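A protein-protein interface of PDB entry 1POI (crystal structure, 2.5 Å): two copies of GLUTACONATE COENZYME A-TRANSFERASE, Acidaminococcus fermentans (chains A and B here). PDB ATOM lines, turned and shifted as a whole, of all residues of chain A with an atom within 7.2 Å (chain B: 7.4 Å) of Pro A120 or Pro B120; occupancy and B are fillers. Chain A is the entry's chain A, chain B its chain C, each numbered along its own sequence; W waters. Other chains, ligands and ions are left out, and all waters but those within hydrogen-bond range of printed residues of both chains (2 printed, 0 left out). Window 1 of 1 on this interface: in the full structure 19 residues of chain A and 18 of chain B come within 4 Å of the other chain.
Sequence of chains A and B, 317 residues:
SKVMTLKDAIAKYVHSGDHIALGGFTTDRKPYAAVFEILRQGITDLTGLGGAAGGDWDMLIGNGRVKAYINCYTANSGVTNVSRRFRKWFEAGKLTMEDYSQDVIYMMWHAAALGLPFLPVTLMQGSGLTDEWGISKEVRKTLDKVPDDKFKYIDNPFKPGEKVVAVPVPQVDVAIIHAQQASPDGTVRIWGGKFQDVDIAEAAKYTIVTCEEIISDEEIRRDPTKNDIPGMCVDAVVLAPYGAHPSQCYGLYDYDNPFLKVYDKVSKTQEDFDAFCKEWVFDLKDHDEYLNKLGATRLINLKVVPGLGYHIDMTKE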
ATOM      1  N   MET A 107      -2.024  14.791  11.273  1.00  0.00           N
ATOM      2  CA  MET A 107      -0.622  14.419  11.447  1.00  0.00           C
ATOM      3  C   MET A 107      -0.544  12.906  11.747  1.00  0.00           C
ATOM      4  O   MET A 107       0.091  12.154  11.002  1.00  0.00           O
ATOM      5  CB  MET A 107       0.043  15.205  12.592  1.00  0.00           C
ATOM      6  CG  MET A 107       0.141  16.700  12.355  1.00  0.00           C
ATOM      7  SD  MET A 107       1.593  17.349  11.489  1.00  0.00           S
ATOM      8  CE  MET A 107       1.997  16.049  10.333  1.00  0.00           C
ATOM      9  N   ALA A 111       1.974  10.567   9.900  1.00  0.00           N
ATOM     10  CA  ALA A 111       3.074   9.853  10.532  1.00  0.00           C
ATOM     11  C   ALA A 111       2.911   8.347  10.338  1.00  0.00           C
ATOM     12  O   ALA A 111       3.898   7.624  10.221  1.00  0.00           O
ATOM     13  CB  ALA A 111       3.120  10.157  11.975  1.00  0.00           C
ATOM     14  N   GLY A 115       5.624   5.947   8.709  1.00  0.00           N
ATOM     15  CA  GLY A 115       6.319   4.878   9.406  1.00  0.00           C
ATOM     16  C   GLY A 115       7.011   5.367  10.667  1.00  0.00           C
ATOM     17  O   GLY A 115       7.920   4.718  11.180  1.00  0.00           O
ATOM     18  N   LEU A 116       6.604   6.516  11.186  1.00  0.00           N
ATOM     19  CA  LEU A 116       7.242   7.040  12.387  1.00  0.00           C
ATOM     20  C   LEU A 116       6.897   6.199  13.614  1.00  0.00           C
ATOM     21  O   LEU A 116       5.802   5.651  13.719  1.00  0.00           O
ATOM     22  CB  LEU A 116       6.822   8.497  12.638  1.00  0.00           C
ATOM     23  CG  LEU A 116       7.036   9.569  11.569  1.00  0.00           C
ATOM     24  CD1 LEU A 116       6.729  10.930  12.169  1.00  0.00           C
ATOM     25  CD2 LEU A 116       8.448   9.565  11.045  1.00  0.00           C
ATOM     26  N   PRO A 117       7.832   6.089  14.565  1.00  0.00           N
ATOM     27  CA  PRO A 117       7.624   5.318  15.799  1.00  0.00           C
ATOM     28  C   PRO A 117       6.425   5.930  16.526  1.00  0.00           C
ATOM     29  O   PRO A 117       5.539   5.240  17.033  1.00  0.00           O
ATOM     30  CB  PRO A 117       8.894   5.609  16.598  1.00  0.00           C
ATOM     31  CG  PRO A 117       9.905   5.892  15.560  1.00  0.00           C
ATOM     32  CD  PRO A 117       9.162   6.713  14.552  1.00  0.00           C
ATOM     33  N   PHE A 118       6.432   7.250  16.586  1.00  0.00           N
ATOM     34  CA  PHE A 118       5.381   8.009  17.235  1.00  0.00           C
ATOM     35  C   PHE A 118       5.433   9.440  16.697  1.00  0.00           C
ATOM     36  O   PHE A 118       6.309   9.783  15.894  1.00  0.00           O
ATOM     37  CB  PHE A 118       5.563   7.970  18.749  1.00  0.00           C
ATOM     38  CG  PHE A 118       6.804   8.649  19.232  1.00  0.00           C
ATOM     39  CD1 PHE A 118       8.035   8.006  19.164  1.00  0.00           C
ATOM     40  CD2 PHE A 118       6.728   9.914  19.831  1.00  0.00           C
ATOM     41  CE1 PHE A 118       9.176   8.606  19.696  1.00  0.00           C
ATOM     42  CE2 PHE A 118       7.859  10.529  20.367  1.00  0.00           C
ATOM     43  CZ  PHE A 118       9.086   9.876  20.303  1.00  0.00           C
ATOM     44  N   LEU A 119       4.533  10.289  17.174  1.00  0.00           N
ATOM     45  CA  LEU A 119       4.491  11.652  16.690  1.00  0.00           C
ATOM     46  C   LEU A 119       4.736  12.741  17.723  1.00  0.00           C
ATOM     47  O   LEU A 119       3.918  12.932  18.623  1.00  0.00           O
ATOM     48  CB  LEU A 119       3.139  11.872  16.001  1.00  0.00           C
ATOM     49  CG  LEU A 119       2.725  13.275  15.558  1.00  0.00           C
ATOM     50  CD1 LEU A 119       3.520  13.709  14.313  1.00  0.00           C
ATOM     51  CD2 LEU A 119       1.245  13.237  15.283  1.00  0.00           C
ATOM     52  N   PRO A 120       5.877  13.451  17.633  1.00  0.00           N
ATOM     53  CA  PRO A 120       6.128  14.520  18.610  1.00  0.00           C
ATOM     54  C   PRO A 120       5.644  15.865  18.010  1.00  0.00           C
ATOM     55  O   PRO A 120       5.989  16.220  16.875  1.00  0.00           O
ATOM     56  CB  PRO A 120       7.651  14.480  18.789  1.00  0.00           C
ATOM     57  CG  PRO A 120       8.167  14.151  17.371  1.00  0.00           C
ATOM     58  CD  PRO A 120       7.056  13.223  16.763  1.00  0.00           C
ATOM     59  N   VAL A 121       4.791  16.575  18.734  1.00  0.00           N
ATOM     60  CA  VAL A 121       4.295  17.841  18.239  1.00  0.00           C
ATOM     61  C   VAL A 121       4.347  18.866  19.330  1.00  0.00           C
ATOM     62  O   VAL A 121       4.243  18.541  20.503  1.00  0.00           O
ATOM     63  CB  VAL A 121       2.805  17.765  17.748  1.00  0.00           C
ATOM     64  CG1 VAL A 121       2.680  16.869  16.530  1.00  0.00           C
ATOM     65  CG2 VAL A 121       1.881  17.309  18.852  1.00  0.00           C
ATOM     66  N   THR A 122       4.513  20.120  18.947  1.00  0.00           N
ATOM     67  CA  THR A 122       4.512  21.193  19.924  1.00  0.00           C
ATOM     68  C   THR A 122       3.084  21.812  19.946  1.00  0.00           C
ATOM     69  O   THR A 122       2.919  23.027  20.080  1.00  0.00           O
ATOM     70  CB  THR A 122       5.566  22.230  19.545  1.00  0.00           C
ATOM     71  OG1 THR A 122       5.962  22.023  18.178  1.00  0.00           O
ATOM     72  CG2 THR A 122       6.768  22.113  20.450  1.00  0.00           C
ATOM     73  N   LEU A 123       2.061  20.956  19.870  1.00  0.00           N
ATOM     74  CA  LEU A 123       0.667  21.400  19.824  1.00  0.00           C
ATOM     75  C   LEU A 123      -0.156  20.740  20.910  1.00  0.00           C
ATOM     76  O   LEU A 123       0.203  19.679  21.395  1.00  0.00           O
ATOM     77  CB  LEU A 123       0.046  21.046  18.455  1.00  0.00           C
ATOM     78  CG  LEU A 123       0.579  21.704  17.174  1.00  0.00           C
ATOM     79  CD1 LEU A 123       0.057  20.999  15.954  1.00  0.00           C
ATOM     80  CD2 LEU A 123       0.214  23.177  17.152  1.00  0.00           C
ATOM     81  N   ILE A 154       7.218  14.681  26.763  1.00  0.00           N
ATOM     82  CA  ILE A 154       8.587  14.206  26.758  1.00  0.00           C
ATOM     83  C   ILE A 154       9.499  15.374  26.517  1.00  0.00           C
ATOM     84  O   ILE A 154       9.075  16.364  25.949  1.00  0.00           O
ATOM     85  CB  ILE A 154       8.806  13.156  25.648  1.00  0.00           C
ATOM     86  CG1 ILE A 154       8.646  13.795  24.264  1.00  0.00           C
ATOM     87  CG2 ILE A 154       7.831  11.994  25.833  1.00  0.00           C
ATOM     88  CD1 ILE A 154       9.124  12.919  23.105  1.00  0.00           C
ATOM     89  N   VAL A 164       7.844  18.354  24.575  1.00  0.00           N
ATOM     90  CA  VAL A 164       6.888  18.277  23.480  1.00  0.00           C
ATOM     91  C   VAL A 164       5.830  17.216  23.861  1.00  0.00           C
ATOM     92  O   VAL A 164       5.990  16.483  24.846  1.00  0.00           O
ATOM     93  CB  VAL A 164       7.597  17.912  22.114  1.00  0.00           C
ATOM     94  CG1 VAL A 164       8.975  18.545  22.035  1.00  0.00           C
ATOM     95  CG2 VAL A 164       7.681  16.399  21.892  1.00  0.00           C
ATOM     96  N   VAL A 165       4.758  17.139  23.087  1.00  0.00           N
ATOM     97  CA  VAL A 165       3.690  16.191  23.328  1.00  0.00           C
ATOM     98  C   VAL A 165       3.908  15.054  22.357  1.00  0.00           C
ATOM     99  O   VAL A 165       4.031  15.290  21.147  1.00  0.00           O
ATOM    100  CB  VAL A 165       2.309  16.852  23.066  1.00  0.00           C
ATOM    101  CG1 VAL A 165       1.178  15.827  23.140  1.00  0.00           C
ATOM    102  CG2 VAL A 165       2.071  17.959  24.076  1.00  0.00           C
ATOM    103  N   ALA A 166       4.054  13.837  22.881  1.00  0.00           N
ATOM    104  CA  ALA A 166       4.260  12.679  22.021  1.00  0.00           C
ATOM    105  C   ALA A 166       2.907  12.030  21.874  1.00  0.00           C
ATOM    106  O   ALA A 166       2.169  11.903  22.860  1.00  0.00           O
ATOM    107  CB  ALA A 166       5.257  11.725  22.629  1.00  0.00           C
ATOM    108  N   VAL A 167       2.585  11.604  20.660  1.00  0.00           N
ATOM    109  CA  VAL A 167       1.287  11.018  20.362  1.00  0.00           C
ATOM    110  C   VAL A 167       1.440   9.667  19.667  1.00  0.00           C
ATOM    111  O   VAL A 167       2.245   9.514  18.759  1.00  0.00           O
ATOM    112  CB  VAL A 167       0.467  12.016  19.478  1.00  0.00           C
ATOM    113  CG1 VAL A 167      -0.644  11.334  18.774  1.00  0.00           C
ATOM    114  CG2 VAL A 167      -0.110  13.106  20.327  1.00  0.00           C
ATOM    115  N   MET B 107      13.520  12.761   4.986  1.00  0.00           N
ATOM    116  CA  MET B 107      12.602  12.839   6.112  1.00  0.00           C
ATOM    117  C   MET B 107      12.927  14.046   6.953  1.00  0.00           C
ATOM    118  O   MET B 107      12.051  14.554   7.643  1.00  0.00           O
ATOM    119  CB  MET B 107      12.687  11.595   6.997  1.00  0.00           C
ATOM    120  CG  MET B 107      12.012  10.339   6.460  1.00  0.00           C
ATOM    121  SD  MET B 107      10.201  10.303   6.614  1.00  0.00           S
ATOM    122  CE  MET B 107       9.871  11.612   7.895  1.00  0.00           C
ATOM    123  N   ALA B 111      10.214  17.002   7.629  1.00  0.00           N
ATOM    124  CA  ALA B 111       9.843  17.199   9.024  1.00  0.00           C
ATOM    125  C   ALA B 111       9.959  18.670   9.334  1.00  0.00           C
ATOM    126  O   ALA B 111       9.295  19.166  10.238  1.00  0.00           O
ATOM    127  CB  ALA B 111      10.762  16.399   9.933  1.00  0.00           C
ATOM    128  N   GLY B 115       6.957  21.131  10.426  1.00  0.00           N
ATOM    129  CA  GLY B 115       7.085  21.794  11.710  1.00  0.00           C
ATOM    130  C   GLY B 115       7.264  20.922  12.937  1.00  0.00           C
ATOM    131  O   GLY B 115       6.983  21.387  14.053  1.00  0.00           O
ATOM    132  N   LEU B 116       7.786  19.698  12.778  1.00  0.00           N
ATOM    133  CA  LEU B 116       7.986  18.799  13.930  1.00  0.00           C
ATOM    134  C   LEU B 116       9.160  19.288  14.787  1.00  0.00           C
ATOM    135  O   LEU B 116      10.155  19.714  14.244  1.00  0.00           O
ATOM    136  CB  LEU B 116       8.273  17.390  13.437  1.00  0.00           C
ATOM    137  CG  LEU B 116       7.269  16.764  12.486  1.00  0.00           C
ATOM    138  CD1 LEU B 116       7.813  15.459  11.943  1.00  0.00           C
ATOM    139  CD2 LEU B 116       5.968  16.521  13.212  1.00  0.00           C
ATOM    140  N   PRO B 117       9.074  19.195  16.128  1.00  0.00           N
ATOM    141  CA  PRO B 117      10.167  19.649  17.004  1.00  0.00           C
ATOM    142  C   PRO B 117      11.468  18.858  16.817  1.00  0.00           C
ATOM    143  O   PRO B 117      12.548  19.315  17.209  1.00  0.00           O
ATOM    144  CB  PRO B 117       9.572  19.505  18.414  1.00  0.00           C
ATOM    145  CG  PRO B 117       8.659  18.364  18.268  1.00  0.00           C
ATOM    146  CD  PRO B 117       7.998  18.570  16.920  1.00  0.00           C
ATOM    147  N   PHE B 118      11.346  17.659  16.262  1.00  0.00           N
ATOM    148  CA  PHE B 118      12.487  16.819  15.942  1.00  0.00           C
ATOM    149  C   PHE B 118      11.920  15.622  15.212  1.00  0.00           C
ATOM    150  O   PHE B 118      10.713  15.460  15.179  1.00  0.00           O
ATOM    151  CB  PHE B 118      13.348  16.433  17.170  1.00  0.00           C
ATOM    152  CG  PHE B 118      12.673  15.513  18.150  1.00  0.00           C
ATOM    153  CD1 PHE B 118      12.767  14.128  18.011  1.00  0.00           C
ATOM    154  CD2 PHE B 118      11.961  16.029  19.222  1.00  0.00           C
ATOM    155  CE1 PHE B 118      12.155  13.276  18.934  1.00  0.00           C
ATOM    156  CE2 PHE B 118      11.345  15.177  20.148  1.00  0.00           C
ATOM    157  CZ  PHE B 118      11.441  13.805  20.006  1.00  0.00           C
ATOM    158  N   LEU B 119      12.767  14.829  14.572  1.00  0.00           N
ATOM    159  CA  LEU B 119      12.303  13.672  13.816  1.00  0.00           C
ATOM    160  C   LEU B 119      12.662  12.372  14.516  1.00  0.00           C
ATOM    161  O   LEU B 119      13.820  12.176  14.857  1.00  0.00           O
ATOM    162  CB  LEU B 119      12.949  13.652  12.417  1.00  0.00           C
ATOM    163  CG  LEU B 119      12.579  12.463  11.516  1.00  0.00           C
ATOM    164  CD1 LEU B 119      11.120  12.555  11.126  1.00  0.00           C
ATOM    165  CD2 LEU B 119      13.435  12.403  10.270  1.00  0.00           C
ATOM    166  N   PRO B 120      11.659  11.544  14.873  1.00  0.00           N
ATOM    167  CA  PRO B 120      11.949  10.263  15.525  1.00  0.00           C
ATOM    168  C   PRO B 120      11.834   9.178  14.456  1.00  0.00           C
ATOM    169  O   PRO B 120      10.829   9.094  13.765  1.00  0.00           O
ATOM    170  CB  PRO B 120      10.825  10.147  16.547  1.00  0.00           C
ATOM    171  CG  PRO B 120       9.676  10.727  15.828  1.00  0.00           C
ATOM    172  CD  PRO B 120      10.260  11.943  15.121  1.00  0.00           C
ATOM    173  N   VAL B 121      12.882   8.394  14.257  1.00  0.00           N
ATOM    174  CA  VAL B 121      12.829   7.322  13.262  1.00  0.00           C
ATOM    175  C   VAL B 121      13.438   6.045  13.815  1.00  0.00           C
ATOM    176  O   VAL B 121      14.218   6.073  14.773  1.00  0.00           O
ATOM    177  CB  VAL B 121      13.608   7.675  11.962  1.00  0.00           C
ATOM    178  CG1 VAL B 121      12.833   8.676  11.134  1.00  0.00           C
ATOM    179  CG2 VAL B 121      15.008   8.204  12.292  1.00  0.00           C
ATOM    180  N   THR B 122      13.050   4.921  13.237  1.00  0.00           N
ATOM    181  CA  THR B 122      13.616   3.648  13.642  1.00  0.00           C
ATOM    182  C   THR B 122      14.400   3.122  12.432  1.00  0.00           C
ATOM    183  O   THR B 122      14.111   2.047  11.860  1.00  0.00           O
ATOM    184  CB  THR B 122      12.545   2.667  14.186  1.00  0.00           C
ATOM    185  OG1 THR B 122      11.477   2.502  13.239  1.00  0.00           O
ATOM    186  CG2 THR B 122      11.985   3.207  15.497  1.00  0.00           C
ATOM    187  N   LEU B 123      15.343   3.968  11.999  1.00  0.00           N
ATOM    188  CA  LEU B 123      16.242   3.697  10.875  1.00  0.00           C
ATOM    189  C   LEU B 123      17.633   4.170  11.322  1.00  0.00           C
ATOM    190  O   LEU B 123      17.736   5.003  12.230  1.00  0.00           O
ATOM    191  CB  LEU B 123      15.794   4.469   9.641  1.00  0.00           C
ATOM    192  CG  LEU B 123      14.564   4.011   8.872  1.00  0.00           C
ATOM    193  CD1 LEU B 123      13.990   5.205   8.139  1.00  0.00           C
ATOM    194  CD2 LEU B 123      14.890   2.868   7.905  1.00  0.00           C
ATOM    195  N   ILE B 154      16.549   7.699  22.096  1.00  0.00           N
ATOM    196  CA  ILE B 154      15.545   7.992  23.106  1.00  0.00           C
ATOM    197  C   ILE B 154      14.583   6.822  23.121  1.00  0.00           C
ATOM    198  O   ILE B 154      14.517   6.043  22.170  1.00  0.00           O
ATOM    199  CB  ILE B 154      14.777   9.325  22.815  1.00  0.00           C
ATOM    200  CG1 ILE B 154      14.076   9.254  21.448  1.00  0.00           C
ATOM    201  CG2 ILE B 154      15.737  10.527  22.896  1.00  0.00           C
ATOM    202  CD1 ILE B 154      12.992  10.283  21.235  1.00  0.00           C
ATOM    203  N   VAL B 164      14.358   4.703  19.957  1.00  0.00           N
ATOM    204  CA  VAL B 164      14.281   5.300  18.638  1.00  0.00           C
ATOM    205  C   VAL B 164      15.398   6.319  18.429  1.00  0.00           C
ATOM    206  O   VAL B 164      15.960   6.859  19.398  1.00  0.00           O
ATOM    207  CB  VAL B 164      12.878   5.939  18.415  1.00  0.00           C
ATOM    208  CG1 VAL B 164      11.789   4.937  18.801  1.00  0.00           C
ATOM    209  CG2 VAL B 164      12.721   7.225  19.211  1.00  0.00           C
ATOM    210  N   VAL B 165      15.746   6.546  17.169  1.00  0.00           N
ATOM    211  CA  VAL B 165      16.785   7.501  16.831  1.00  0.00           C
ATOM    212  C   VAL B 165      16.181   8.879  16.509  1.00  0.00           C
ATOM    213  O   VAL B 165      15.560   9.060  15.457  1.00  0.00           O
ATOM    214  CB  VAL B 165      17.619   6.994  15.629  1.00  0.00           C
ATOM    215  CG1 VAL B 165      18.694   8.004  15.245  1.00  0.00           C
ATOM    216  CG2 VAL B 165      18.257   5.670  15.976  1.00  0.00           C
ATOM    217  N   ALA B 166      16.310   9.806  17.457  1.00  0.00           N
ATOM    218  CA  ALA B 166      15.850  11.185  17.323  1.00  0.00           C
ATOM    219  C   ALA B 166      16.892  12.027  16.537  1.00  0.00           C
ATOM    220  O   ALA B 166      17.995  12.297  17.041  1.00  0.00           O
ATOM    221  CB  ALA B 166      15.645  11.786  18.695  1.00  0.00           C
ATOM    222  N   VAL B 167      16.547  12.440  15.317  1.00  0.00           N
ATOM    223  CA  VAL B 167      17.437  13.246  14.466  1.00  0.00           C
ATOM    224  C   VAL B 167      17.022  14.721  14.604  1.00  0.00           C
ATOM    225  O   VAL B 167      15.835  15.006  14.778  1.00  0.00           O
ATOM    226  CB  VAL B 167      17.310  12.809  12.997  1.00  0.00           C
ATOM    227  CG1 VAL B 167      18.371  13.451  12.152  1.00  0.00           C
ATOM    228  CG2 VAL B 167      17.423  11.330  12.886  1.00  0.00           C
ATOM    229  N   VAL B 169      16.063  18.513  13.451  1.00  0.00           N
ATOM    230  CA  VAL B 169      15.439  19.017  12.209  1.00  0.00           C
ATOM    231  C   VAL B 169      16.191  20.230  11.627  1.00  0.00           C
ATOM    232  O   VAL B 169      16.568  21.146  12.360  1.00  0.00           O
ATOM    233  CB  VAL B 169      13.932  19.314  12.415  1.00  0.00           C
ATOM    234  CG1 VAL B 169      13.301  19.745  11.120  1.00  0.00           C
ATOM    235  CG2 VAL B 169      13.205  18.050  12.877  1.00  0.00           C
HETATM  236  O   HOH W   1       4.490  20.539  15.427  1.00  0.00           O
HETATM  237  O   HOH W   2       8.961   3.106  13.296  1.00  0.00           O
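O of Ile B154 sits at hydrogen-bond distance from N of Val B164 (2.6 Å). The backbone carbonyl oxygen (O) of Leu A119 sits at hydrogen-bond distance from the backbone NH (N) of Val A167, at 2.8 Å. The backbone carbonyl oxygen of Ala B111 lies within hydrogen-bond range of the backbone NH of Leu B116 (3.0 Å). N of Val A121 is in hydrogen-bond range of O of Val A165, 2.8 Å away. The backbone NH (N) of Val A164 sits at hydrogen-bond distance from the backbone carbonyl oxygen (O) of Ile A154 (2.7 Å). The backbone carbonyl oxygen of Val B121 is in hydrogen-bond range of the backbone NH of Val B165 (2.9 Å).
Among the printed residues, merely in contact across the chains: Pro A117 with Pro B120, Pro A120 with Pro B117, Pro A117 with Thr B122, Phe A118 with Pro B120, Pro A120 with Phe B118, Leu A116 with Pro B120, Pro A120 with Leu B116, Pro A117 with Val B164, Pro A120 with Pro B120, Val A164 with Pro B117, Phe A118 with Val B164, Leu A119 with Leu B116, Pro A117 with Val B121, Ile A154 with Phe B118 and Val A121 with Pro B117.
Of the printed residues of chain A, Pro B120 touches Leu A116 (3.6 Å), Pro A117 (3.0 Å), Phe A118 (3.5 Å) and Pro A120 (3.7 Å). Of the printed residues of chain B, Leu A116 touches Pro B120 (3.6 Å). Of the printed residues of chain A, Phe B118 touches Pro A120 (3.6 Å) and Ile A154 (3.97 Å). Of the printed residues of chain B, Pro A117 touches Pro B120, Val B121, Thr B122 and Val B164.
Of the 16 printed residues of chain A, 8 touch a printed residue of chain B. Printed residues of chain A that touch a printed residue of chain B: Leu A116, Pro A117, Phe A118, Leu A119, Pro A120, Val A121, Ile A154 and Val A164. Of the 17 printed residues of chain B, 7 touch a printed residue of chain A. Hydrophobic or aromatic side chains of chain B that line the printed part of chain A: Leu B116, Pro B117, Phe B118, Pro B120 and Val B164. Along chain B the printed residues that touch a printed residue of chain A span positions 116 to 164.
Leu A116 touches Pro B120, and with the chains exchanged Pro A120 touches Leu B116. Pro A117 touches Thr B122, but with the chains exchanged Thr A122 does not touch Pro B117 (4.2 Å). Phe A118 touches Pro B120, and with the chains exchanged Pro A120 touches Phe B118. Pro B120 touches its own counterpart, Pro A120. 16 positions are printed for both chains. Of the 15 pairs that touch across the chains among the printed residues, 11 have their exchanged pair printed and touching as well.
Water W2 lies within hydrogen-bond range of the side-chain hydroxyl of Thr B122 and the backbone carbonyl oxygen of Gly A115. Water W1 lies within hydrogen-bond range of the backbone carbonyl oxygen of Gly B115 (3.0 Å) and the side-chain hydroxyl of Thr A122 (3.5 Å).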
